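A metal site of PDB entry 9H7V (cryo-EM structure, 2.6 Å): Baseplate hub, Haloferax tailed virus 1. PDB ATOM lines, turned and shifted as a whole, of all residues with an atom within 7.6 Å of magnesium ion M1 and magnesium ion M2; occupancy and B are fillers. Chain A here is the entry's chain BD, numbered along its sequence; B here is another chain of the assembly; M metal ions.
Ala 47 touches magnesium ion M1 (O to MG, 3.6 Å). Gly 51 touches magnesium ion M1 (C to MG, 3.9 Å). Along chain A the residues within 4 Å of magnesium ion M1 span positions 46 to 116. The nearest printed residue that does not touch magnesium ion M1 is Arg 120 (4.2 Å).
N of Ser 114 is in hydrogen-bond range of O of Asp 52, at 3.4 Å. The backbone carbonyl oxygen of Phe 50 sits close to the guanidinium group of Arg 120 (3.2 Å). The backbone NH of Ala 47 is in hydrogen-bond range of the backbone carbonyl oxygen of Ala 328, at 3.2 Å. OD2 of Asp 45 lies within salt-bridge range of NH1 of Arg 89. The side-chain carboxylate (OD1) of Asp 116 lies within salt-bridge range of the guanidinium group (NH2) of Arg 120 (3.1 Å).
Magnesium ion M2 is bound by the side-chain carboxylate of Asp 45 (2.2 Å) and the side-chain carboxylate of Asp 52 (2.5 Å). Magnesium ion M2 has two donor atoms within binding distance.
Three residues have an atom within 4 Å of magnesium ion M2: Asp 45, Thr 46 and Asp 52.
Magnesium ion M1 is bound by OD2 of Asp 116 (2.0 Å). Magnesium ion M1 is bound by OD1 of Asp 52, 2.1 Å away. The backbone carbonyl oxygen (O) of Phe 50 is bound to magnesium ion M1 (2.1 Å). Magnesium ion M1 is bound by the backbone carbonyl oxygen (O) of Thr 46 (2.1 Å).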
ATOM      1  N   VAL A  44     -10.714  19.558 -15.058  1.00  0.00           N
ATOM      2  CA  VAL A  44     -11.624  18.512 -15.502  1.00  0.00           C
ATOM      3  C   VAL A  44     -11.097  17.908 -16.798  1.00  0.00           C
ATOM      4  O   VAL A  44     -10.812  18.620 -17.756  1.00  0.00           O
ATOM      5  CB  VAL A  44     -13.075  19.018 -15.628  1.00  0.00           C
ATOM      6  CG1 VAL A  44     -14.025  17.916 -16.088  1.00  0.00           C
ATOM      7  CG2 VAL A  44     -13.578  19.619 -14.326  1.00  0.00           C
ATOM      8  N   ASP A  45     -10.979  16.571 -16.793  1.00  0.00           N
ATOM      9  CA  ASP A  45     -10.525  15.775 -17.923  1.00  0.00           C
ATOM     10  C   ASP A  45     -11.601  14.747 -18.231  1.00  0.00           C
ATOM     11  O   ASP A  45     -11.897  13.903 -17.393  1.00  0.00           O
ATOM     12  CB  ASP A  45      -9.171  15.127 -17.585  1.00  0.00           C
ATOM     13  CG  ASP A  45      -8.447  14.479 -18.752  1.00  0.00           C
ATOM     14  OD1 ASP A  45      -8.940  14.599 -19.900  1.00  0.00           O
ATOM     15  OD2 ASP A  45      -7.396  13.858 -18.512  1.00  0.00           O
ATOM     16  N   THR A  46     -12.192  14.832 -19.438  1.00  0.00           N
ATOM     17  CA  THR A  46     -13.454  14.143 -19.696  1.00  0.00           C
ATOM     18  C   THR A  46     -13.572  13.690 -21.154  1.00  0.00           C
ATOM     19  O   THR A  46     -13.152  14.404 -22.073  1.00  0.00           O
ATOM     20  CB  THR A  46     -14.645  14.961 -19.185  1.00  0.00           C
ATOM     21  OG1 THR A  46     -15.861  14.254 -19.447  1.00  0.00           O
ATOM     22  CG2 THR A  46     -14.721  16.363 -19.771  1.00  0.00           C
ATOM     23  N   ALA A  47     -14.198  12.516 -21.318  1.00  0.00           N
ATOM     24  CA  ALA A  47     -14.385  11.801 -22.580  1.00  0.00           C
ATOM     25  C   ALA A  47     -15.187  12.644 -23.574  1.00  0.00           C
ATOM     26  O   ALA A  47     -15.843  13.615 -23.186  1.00  0.00           O
ATOM     27  CB  ALA A  47     -15.037  10.467 -22.315  1.00  0.00           C
ATOM     28  N   ASN A  48     -15.182  12.195 -24.838  1.00  0.00           N
ATOM     29  CA  ASN A  48     -15.315  13.033 -26.023  1.00  0.00           C
ATOM     30  C   ASN A  48     -16.555  13.937 -26.041  1.00  0.00           C
ATOM     31  O   ASN A  48     -16.398  15.092 -26.433  1.00  0.00           O
ATOM     32  CB  ASN A  48     -15.098  12.244 -27.321  1.00  0.00           C
ATOM     33  CG  ASN A  48     -13.649  11.880 -27.525  1.00  0.00           C
ATOM     34  OD1 ASN A  48     -12.800  12.759 -27.690  1.00  0.00           O
ATOM     35  ND2 ASN A  48     -13.362  10.594 -27.505  1.00  0.00           N
ATOM     36  N   PRO A  49     -17.787  13.491 -25.685  1.00  0.00           N
ATOM     37  CA  PRO A  49     -18.947  14.394 -25.726  1.00  0.00           C
ATOM     38  C   PRO A  49     -18.785  15.682 -24.908  1.00  0.00           C
ATOM     39  O   PRO A  49     -19.520  16.638 -25.121  1.00  0.00           O
ATOM     40  CB  PRO A  49     -20.088  13.548 -25.148  1.00  0.00           C
ATOM     41  CG  PRO A  49     -19.666  12.124 -25.416  1.00  0.00           C
ATOM     42  CD  PRO A  49     -18.159  12.128 -25.277  1.00  0.00           C
ATOM     43  N   PHE A  50     -17.788  15.692 -24.009  1.00  0.00           N
ATOM     44  CA  PHE A  50     -17.670  16.718 -22.978  1.00  0.00           C
ATOM     45  C   PHE A  50     -16.322  17.446 -23.070  1.00  0.00           C
ATOM     46  O   PHE A  50     -15.298  16.834 -23.359  1.00  0.00           O
ATOM     47  CB  PHE A  50     -17.885  16.113 -21.597  1.00  0.00           C
ATOM     48  CG  PHE A  50     -19.254  15.505 -21.398  1.00  0.00           C
ATOM     49  CD1 PHE A  50     -20.342  16.302 -21.075  1.00  0.00           C
ATOM     50  CD2 PHE A  50     -19.448  14.144 -21.553  1.00  0.00           C
ATOM     51  CE1 PHE A  50     -21.593  15.746 -20.904  1.00  0.00           C
ATOM     52  CE2 PHE A  50     -20.709  13.586 -21.380  1.00  0.00           C
ATOM     53  CZ  PHE A  50     -21.788  14.396 -21.050  1.00  0.00           C
ATOM     54  N   GLY A  51     -16.368  18.753 -22.774  1.00  0.00           N
ATOM     55  CA  GLY A  51     -15.223  19.629 -22.885  1.00  0.00           C
ATOM     56  C   GLY A  51     -14.329  19.584 -21.642  1.00  0.00           C
ATOM     57  O   GLY A  51     -14.820  19.719 -20.525  1.00  0.00           O
ATOM     58  N   ASP A  52     -13.023  19.385 -21.868  1.00  0.00           N
ATOM     59  CA  ASP A  52     -12.012  19.488 -20.832  1.00  0.00           C
ATOM     60  C   ASP A  52     -11.812  20.964 -20.501  1.00  0.00           C
ATOM     61  O   ASP A  52     -11.650  21.783 -21.404  1.00  0.00           O
ATOM     62  CB  ASP A  52     -10.695  18.851 -21.268  1.00  0.00           C
ATOM     63  CG  ASP A  52     -10.771  17.384 -21.652  1.00  0.00           C
ATOM     64  OD1 ASP A  52     -11.900  16.854 -21.772  1.00  0.00           O
ATOM     65  OD2 ASP A  52      -9.704  16.776 -21.826  1.00  0.00           O
ATOM     66  N   TYR A  53     -11.830  21.288 -19.204  1.00  0.00           N
ATOM     67  CA  TYR A  53     -11.701  22.670 -18.775  1.00  0.00           C
ATOM     68  C   TYR A  53     -10.939  22.784 -17.453  1.00  0.00           C
ATOM     69  O   TYR A  53     -10.861  21.820 -16.700  1.00  0.00           O
ATOM     70  CB  TYR A  53     -13.070  23.366 -18.719  1.00  0.00           C
ATOM     71  CG  TYR A  53     -13.974  22.986 -17.566  1.00  0.00           C
ATOM     72  CD1 TYR A  53     -14.736  21.829 -17.597  1.00  0.00           C
ATOM     73  CD2 TYR A  53     -14.090  23.806 -16.454  1.00  0.00           C
ATOM     74  CE1 TYR A  53     -15.578  21.487 -16.553  1.00  0.00           C
ATOM     75  CE2 TYR A  53     -14.923  23.479 -15.393  1.00  0.00           C
ATOM     76  CZ  TYR A  53     -15.676  22.311 -15.445  1.00  0.00           C
ATOM     77  OH  TYR A  53     -16.494  21.985 -14.417  1.00  0.00           O
ATOM     78  N   ARG A  89      -0.651  18.488 -16.046  1.00  0.00           N
ATOM     79  CA  ARG A  89      -1.917  17.779 -15.992  1.00  0.00           C
ATOM     80  C   ARG A  89      -2.973  18.410 -16.900  1.00  0.00           C
ATOM     81  O   ARG A  89      -3.892  17.718 -17.337  1.00  0.00           O
ATOM     82  CB  ARG A  89      -2.406  17.615 -14.542  1.00  0.00           C
ATOM     83  CG  ARG A  89      -3.545  16.612 -14.360  1.00  0.00           C
ATOM     84  CD  ARG A  89      -3.243  15.252 -14.967  1.00  0.00           C
ATOM     85  NE  ARG A  89      -4.364  14.318 -15.066  1.00  0.00           N
ATOM     86  CZ  ARG A  89      -5.268  14.295 -16.041  1.00  0.00           C
ATOM     87  NH1 ARG A  89      -6.232  13.389 -16.006  1.00  0.00           N
ATOM     88  NH2 ARG A  89      -5.233  15.173 -17.025  1.00  0.00           N
ATOM     89  N   SER A 114      -9.568  23.256 -23.661  1.00  0.00           N
ATOM     90  CA  SER A 114      -8.454  22.477 -24.186  1.00  0.00           C
ATOM     91  C   SER A 114      -8.697  22.061 -25.640  1.00  0.00           C
ATOM     92  O   SER A 114      -9.534  22.644 -26.320  1.00  0.00           O
ATOM     93  CB  SER A 114      -8.151  21.302 -23.283  1.00  0.00           C
ATOM     94  OG  SER A 114      -6.870  20.753 -23.574  1.00  0.00           O
ATOM     95  N   PHE A 115      -7.949  21.046 -26.097  1.00  0.00           N
ATOM     96  CA  PHE A 115      -7.773  20.714 -27.511  1.00  0.00           C
ATOM     97  C   PHE A 115      -8.996  20.041 -28.115  1.00  0.00           C
ATOM     98  O   PHE A 115      -9.128  20.017 -29.341  1.00  0.00           O
ATOM     99  CB  PHE A 115      -6.522  19.862 -27.728  1.00  0.00           C
ATOM    100  CG  PHE A 115      -5.250  20.506 -27.230  1.00  0.00           C
ATOM    101  CD1 PHE A 115      -4.652  21.534 -27.951  1.00  0.00           C
ATOM    102  CD2 PHE A 115      -4.681  20.100 -26.030  1.00  0.00           C
ATOM    103  CE1 PHE A 115      -3.490  22.133 -27.478  1.00  0.00           C
ATOM    104  CE2 PHE A 115      -3.523  20.707 -25.568  1.00  0.00           C
ATOM    105  CZ  PHE A 115      -2.931  21.723 -26.286  1.00  0.00           C
ATOM    106  N   ASP A 116      -9.889  19.495 -27.277  1.00  0.00           N
ATOM    107  CA  ASP A 116     -11.055  18.777 -27.771  1.00  0.00           C
ATOM    108  C   ASP A 116     -12.043  19.737 -28.434  1.00  0.00           C
ATOM    109  O   ASP A 116     -12.941  19.303 -29.151  1.00  0.00           O
ATOM    110  CB  ASP A 116     -11.617  17.759 -26.760  1.00  0.00           C
ATOM    111  CG  ASP A 116     -12.241  18.311 -25.491  1.00  0.00           C
ATOM    112  OD1 ASP A 116     -12.249  19.544 -25.303  1.00  0.00           O
ATOM    113  OD2 ASP A 116     -12.726  17.483 -24.677  1.00  0.00           O
ATOM    114  N   GLN A 117     -11.832  21.048 -28.213  1.00  0.00           N
ATOM    115  CA  GLN A 117     -12.623  22.113 -28.812  1.00  0.00           C
ATOM    116  C   GLN A 117     -12.458  22.134 -30.330  1.00  0.00           C
ATOM    117  O   GLN A 117     -13.401  22.506 -31.032  1.00  0.00           O
ATOM    118  CB  GLN A 117     -12.259  23.469 -28.202  1.00  0.00           C
ATOM    119  CG  GLN A 117     -12.732  23.664 -26.770  1.00  0.00           C
ATOM    120  CD  GLN A 117     -14.230  23.603 -26.584  1.00  0.00           C
ATOM    121  OE1 GLN A 117     -15.005  24.030 -27.424  1.00  0.00           O
ATOM    122  NE2 GLN A 117     -14.649  23.060 -25.445  1.00  0.00           N
ATOM    123  N   ARG A 120     -14.557  19.643 -32.116  1.00  0.00           N
ATOM    124  CA  ARG A 120     -15.945  19.943 -31.799  1.00  0.00           C
ATOM    125  C   ARG A 120     -16.458  21.080 -32.692  1.00  0.00           C
ATOM    126  O   ARG A 120     -17.598  21.044 -33.143  1.00  0.00           O
ATOM    127  CB  ARG A 120     -15.995  20.360 -30.328  1.00  0.00           C
ATOM    128  CG  ARG A 120     -17.384  20.401 -29.694  1.00  0.00           C
ATOM    129  CD  ARG A 120     -17.280  20.395 -28.182  1.00  0.00           C
ATOM    130  NE  ARG A 120     -16.761  19.123 -27.689  1.00  0.00           N
ATOM    131  CZ  ARG A 120     -15.783  18.960 -26.801  1.00  0.00           C
ATOM    132  NH1 ARG A 120     -15.414  17.744 -26.446  1.00  0.00           N
ATOM    133  NH2 ARG A 120     -15.189  20.010 -26.243  1.00  0.00           N
ATOM    134  N   GLU A 172     -16.238  15.615 -34.336  1.00  0.00           N
ATOM    135  CA  GLU A 172     -16.446  14.793 -33.147  1.00  0.00           C
ATOM    136  C   GLU A 172     -17.634  13.852 -33.326  1.00  0.00           C
ATOM    137  O   GLU A 172     -17.580  12.701 -32.878  1.00  0.00           O
ATOM    138  CB  GLU A 172     -16.593  15.699 -31.921  1.00  0.00           C
ATOM    139  CG  GLU A 172     -16.646  14.958 -30.596  1.00  0.00           C
ATOM    140  CD  GLU A 172     -17.164  15.830 -29.467  1.00  0.00           C
ATOM    141  OE1 GLU A 172     -16.399  16.672 -28.966  1.00  0.00           O
ATOM    142  OE2 GLU A 172     -18.358  15.677 -29.112  1.00  0.00           O
ATOM    143  N   PHE A 187     -11.087   8.000 -28.861  1.00  0.00           N
ATOM    144  CA  PHE A 187     -10.368   8.969 -29.686  1.00  0.00           C
ATOM    145  C   PHE A 187     -10.124  10.246 -28.890  1.00  0.00           C
ATOM    146  O   PHE A 187     -10.681  10.441 -27.813  1.00  0.00           O
ATOM    147  CB  PHE A 187     -11.091   9.211 -31.019  1.00  0.00           C
ATOM    148  CG  PHE A 187     -12.453   9.842 -30.912  1.00  0.00           C
ATOM    149  CD1 PHE A 187     -12.603  11.227 -30.960  1.00  0.00           C
ATOM    150  CD2 PHE A 187     -13.590   9.063 -30.787  1.00  0.00           C
ATOM    151  CE1 PHE A 187     -13.859  11.803 -30.873  1.00  0.00           C
ATOM    152  CE2 PHE A 187     -14.845   9.640 -30.689  1.00  0.00           C
ATOM    153  CZ  PHE A 187     -14.980  11.009 -30.737  1.00  0.00           C
ATOM    154  N   GLY A 188      -9.268  11.105 -29.453  1.00  0.00           N
ATOM    155  CA  GLY A 188      -9.005  12.416 -28.881  1.00  0.00           C
ATOM    156  C   GLY A 188      -7.643  12.956 -29.304  1.00  0.00           C
ATOM    157  O   GLY A 188      -6.996  12.410 -30.198  1.00  0.00           O
ATOM    158  N   VAL A 189      -7.236  14.037 -28.638  1.00  0.00           N
ATOM    159  CA  VAL A 189      -5.950  14.671 -28.848  1.00  0.00           C
ATOM    160  C   VAL A 189      -5.116  14.422 -27.593  1.00  0.00           C
ATOM    161  O   VAL A 189      -5.520  14.780 -26.485  1.00  0.00           O
ATOM    162  CB  VAL A 189      -6.099  16.178 -29.141  1.00  0.00           C
ATOM    163  CG1 VAL A 189      -4.769  16.834 -29.464  1.00  0.00           C
ATOM    164  CG2 VAL A 189      -7.099  16.447 -30.248  1.00  0.00           C
ATOM    165  N   ASP A 191      -1.445  14.730 -25.235  1.00  0.00           N
ATOM    166  CA  ASP A 191      -0.676  15.848 -24.717  1.00  0.00           C
ATOM    167  C   ASP A 191       0.323  16.351 -25.761  1.00  0.00           C
ATOM    168  O   ASP A 191       0.712  17.514 -25.740  1.00  0.00           O
ATOM    169  CB  ASP A 191       0.034  15.473 -23.412  1.00  0.00           C
ATOM    170  CG  ASP A 191      -0.879  15.080 -22.265  1.00  0.00           C
ATOM    171  OD1 ASP A 191      -2.060  15.500 -22.269  1.00  0.00           O
ATOM    172  OD2 ASP A 191      -0.412  14.350 -21.367  1.00  0.00           O
ATOM    173  N   PHE A 196      -5.392  10.378 -31.716  1.00  0.00           N
ATOM    174  CA  PHE A 196      -5.404   8.935 -31.560  1.00  0.00           C
ATOM    175  C   PHE A 196      -6.816   8.395 -31.785  1.00  0.00           C
ATOM    176  O   PHE A 196      -7.791   9.100 -31.549  1.00  0.00           O
ATOM    177  CB  PHE A 196      -4.828   8.506 -30.204  1.00  0.00           C
ATOM    178  CG  PHE A 196      -5.639   8.924 -28.996  1.00  0.00           C
ATOM    179  CD1 PHE A 196      -6.651   8.116 -28.507  1.00  0.00           C
ATOM    180  CD2 PHE A 196      -5.367  10.111 -28.334  1.00  0.00           C
ATOM    181  CE1 PHE A 196      -7.400   8.500 -27.397  1.00  0.00           C
ATOM    182  CE2 PHE A 196      -6.107  10.497 -27.226  1.00  0.00           C
ATOM    183  CZ  PHE A 196      -7.122   9.687 -26.757  1.00  0.00           C
ATOM    184  N   GLU A 307      -6.353   8.927 -16.468  1.00  0.00           N
ATOM    185  CA  GLU A 307      -7.035   9.594 -17.567  1.00  0.00           C
ATOM    186  C   GLU A 307      -8.402   8.943 -17.772  1.00  0.00           C
ATOM    187  O   GLU A 307      -8.610   7.821 -17.326  1.00  0.00           O
ATOM    188  CB  GLU A 307      -6.204   9.490 -18.837  1.00  0.00           C
ATOM    189  CG  GLU A 307      -5.012  10.439 -18.886  1.00  0.00           C
ATOM    190  CD  GLU A 307      -4.184  10.386 -20.153  1.00  0.00           C
ATOM    191  OE1 GLU A 307      -4.775  10.212 -21.238  1.00  0.00           O
ATOM    192  OE2 GLU A 307      -2.951  10.516 -20.050  1.00  0.00           O
ATOM    193  N   PRO A 308      -9.377   9.613 -18.443  1.00  0.00           N
ATOM    194  CA  PRO A 308     -10.573   8.928 -18.938  1.00  0.00           C
ATOM    195  C   PRO A 308     -10.184   7.892 -19.979  1.00  0.00           C
ATOM    196  O   PRO A 308      -9.299   8.124 -20.808  1.00  0.00           O
ATOM    197  CB  PRO A 308     -11.451  10.043 -19.530  1.00  0.00           C
ATOM    198  CG  PRO A 308     -10.489  11.187 -19.776  1.00  0.00           C
ATOM    199  CD  PRO A 308      -9.420  11.058 -18.713  1.00  0.00           C
ATOM    200  N   ALA A 328     -14.801   7.607 -16.953  1.00  0.00           N
ATOM    201  CA  ALA A 328     -15.428   8.446 -17.965  1.00  0.00           C
ATOM    202  C   ALA A 328     -14.924   9.882 -17.852  1.00  0.00           C
ATOM    203  O   ALA A 328     -14.815  10.580 -18.862  1.00  0.00           O
ATOM    204  CB  ALA A 328     -16.921   8.371 -17.829  1.00  0.00           C
ATOM    205  N   ARG B 338     -19.124  24.656 -23.311  1.00  0.00           N
ATOM    206  CA  ARG B 338     -18.072  23.666 -23.392  1.00  0.00           C
ATOM    207  C   ARG B 338     -18.315  22.696 -24.544  1.00  0.00           C
ATOM    208  O   ARG B 338     -17.371  22.118 -25.072  1.00  0.00           O
ATOM    209  CB  ARG B 338     -17.970  22.896 -22.068  1.00  0.00           C
ATOM    210  CG  ARG B 338     -16.854  23.383 -21.150  1.00  0.00           C
ATOM    211  CD  ARG B 338     -17.285  23.520 -19.695  1.00  0.00           C
ATOM    212  NE  ARG B 338     -17.840  22.300 -19.115  1.00  0.00           N
ATOM    213  CZ  ARG B 338     -18.477  22.230 -17.952  1.00  0.00           C
ATOM    214  NH1 ARG B 338     -18.930  21.066 -17.521  1.00  0.00           N
ATOM    215  NH2 ARG B 338     -18.657  23.315 -17.210  1.00  0.00           N
HETATM  216 MG    MG M   1     -13.284  16.211 -23.216  1.00  0.00          MG
HETATM  217 MG    MG M   2      -9.176  14.384 -22.125  1.00  0.00          MG
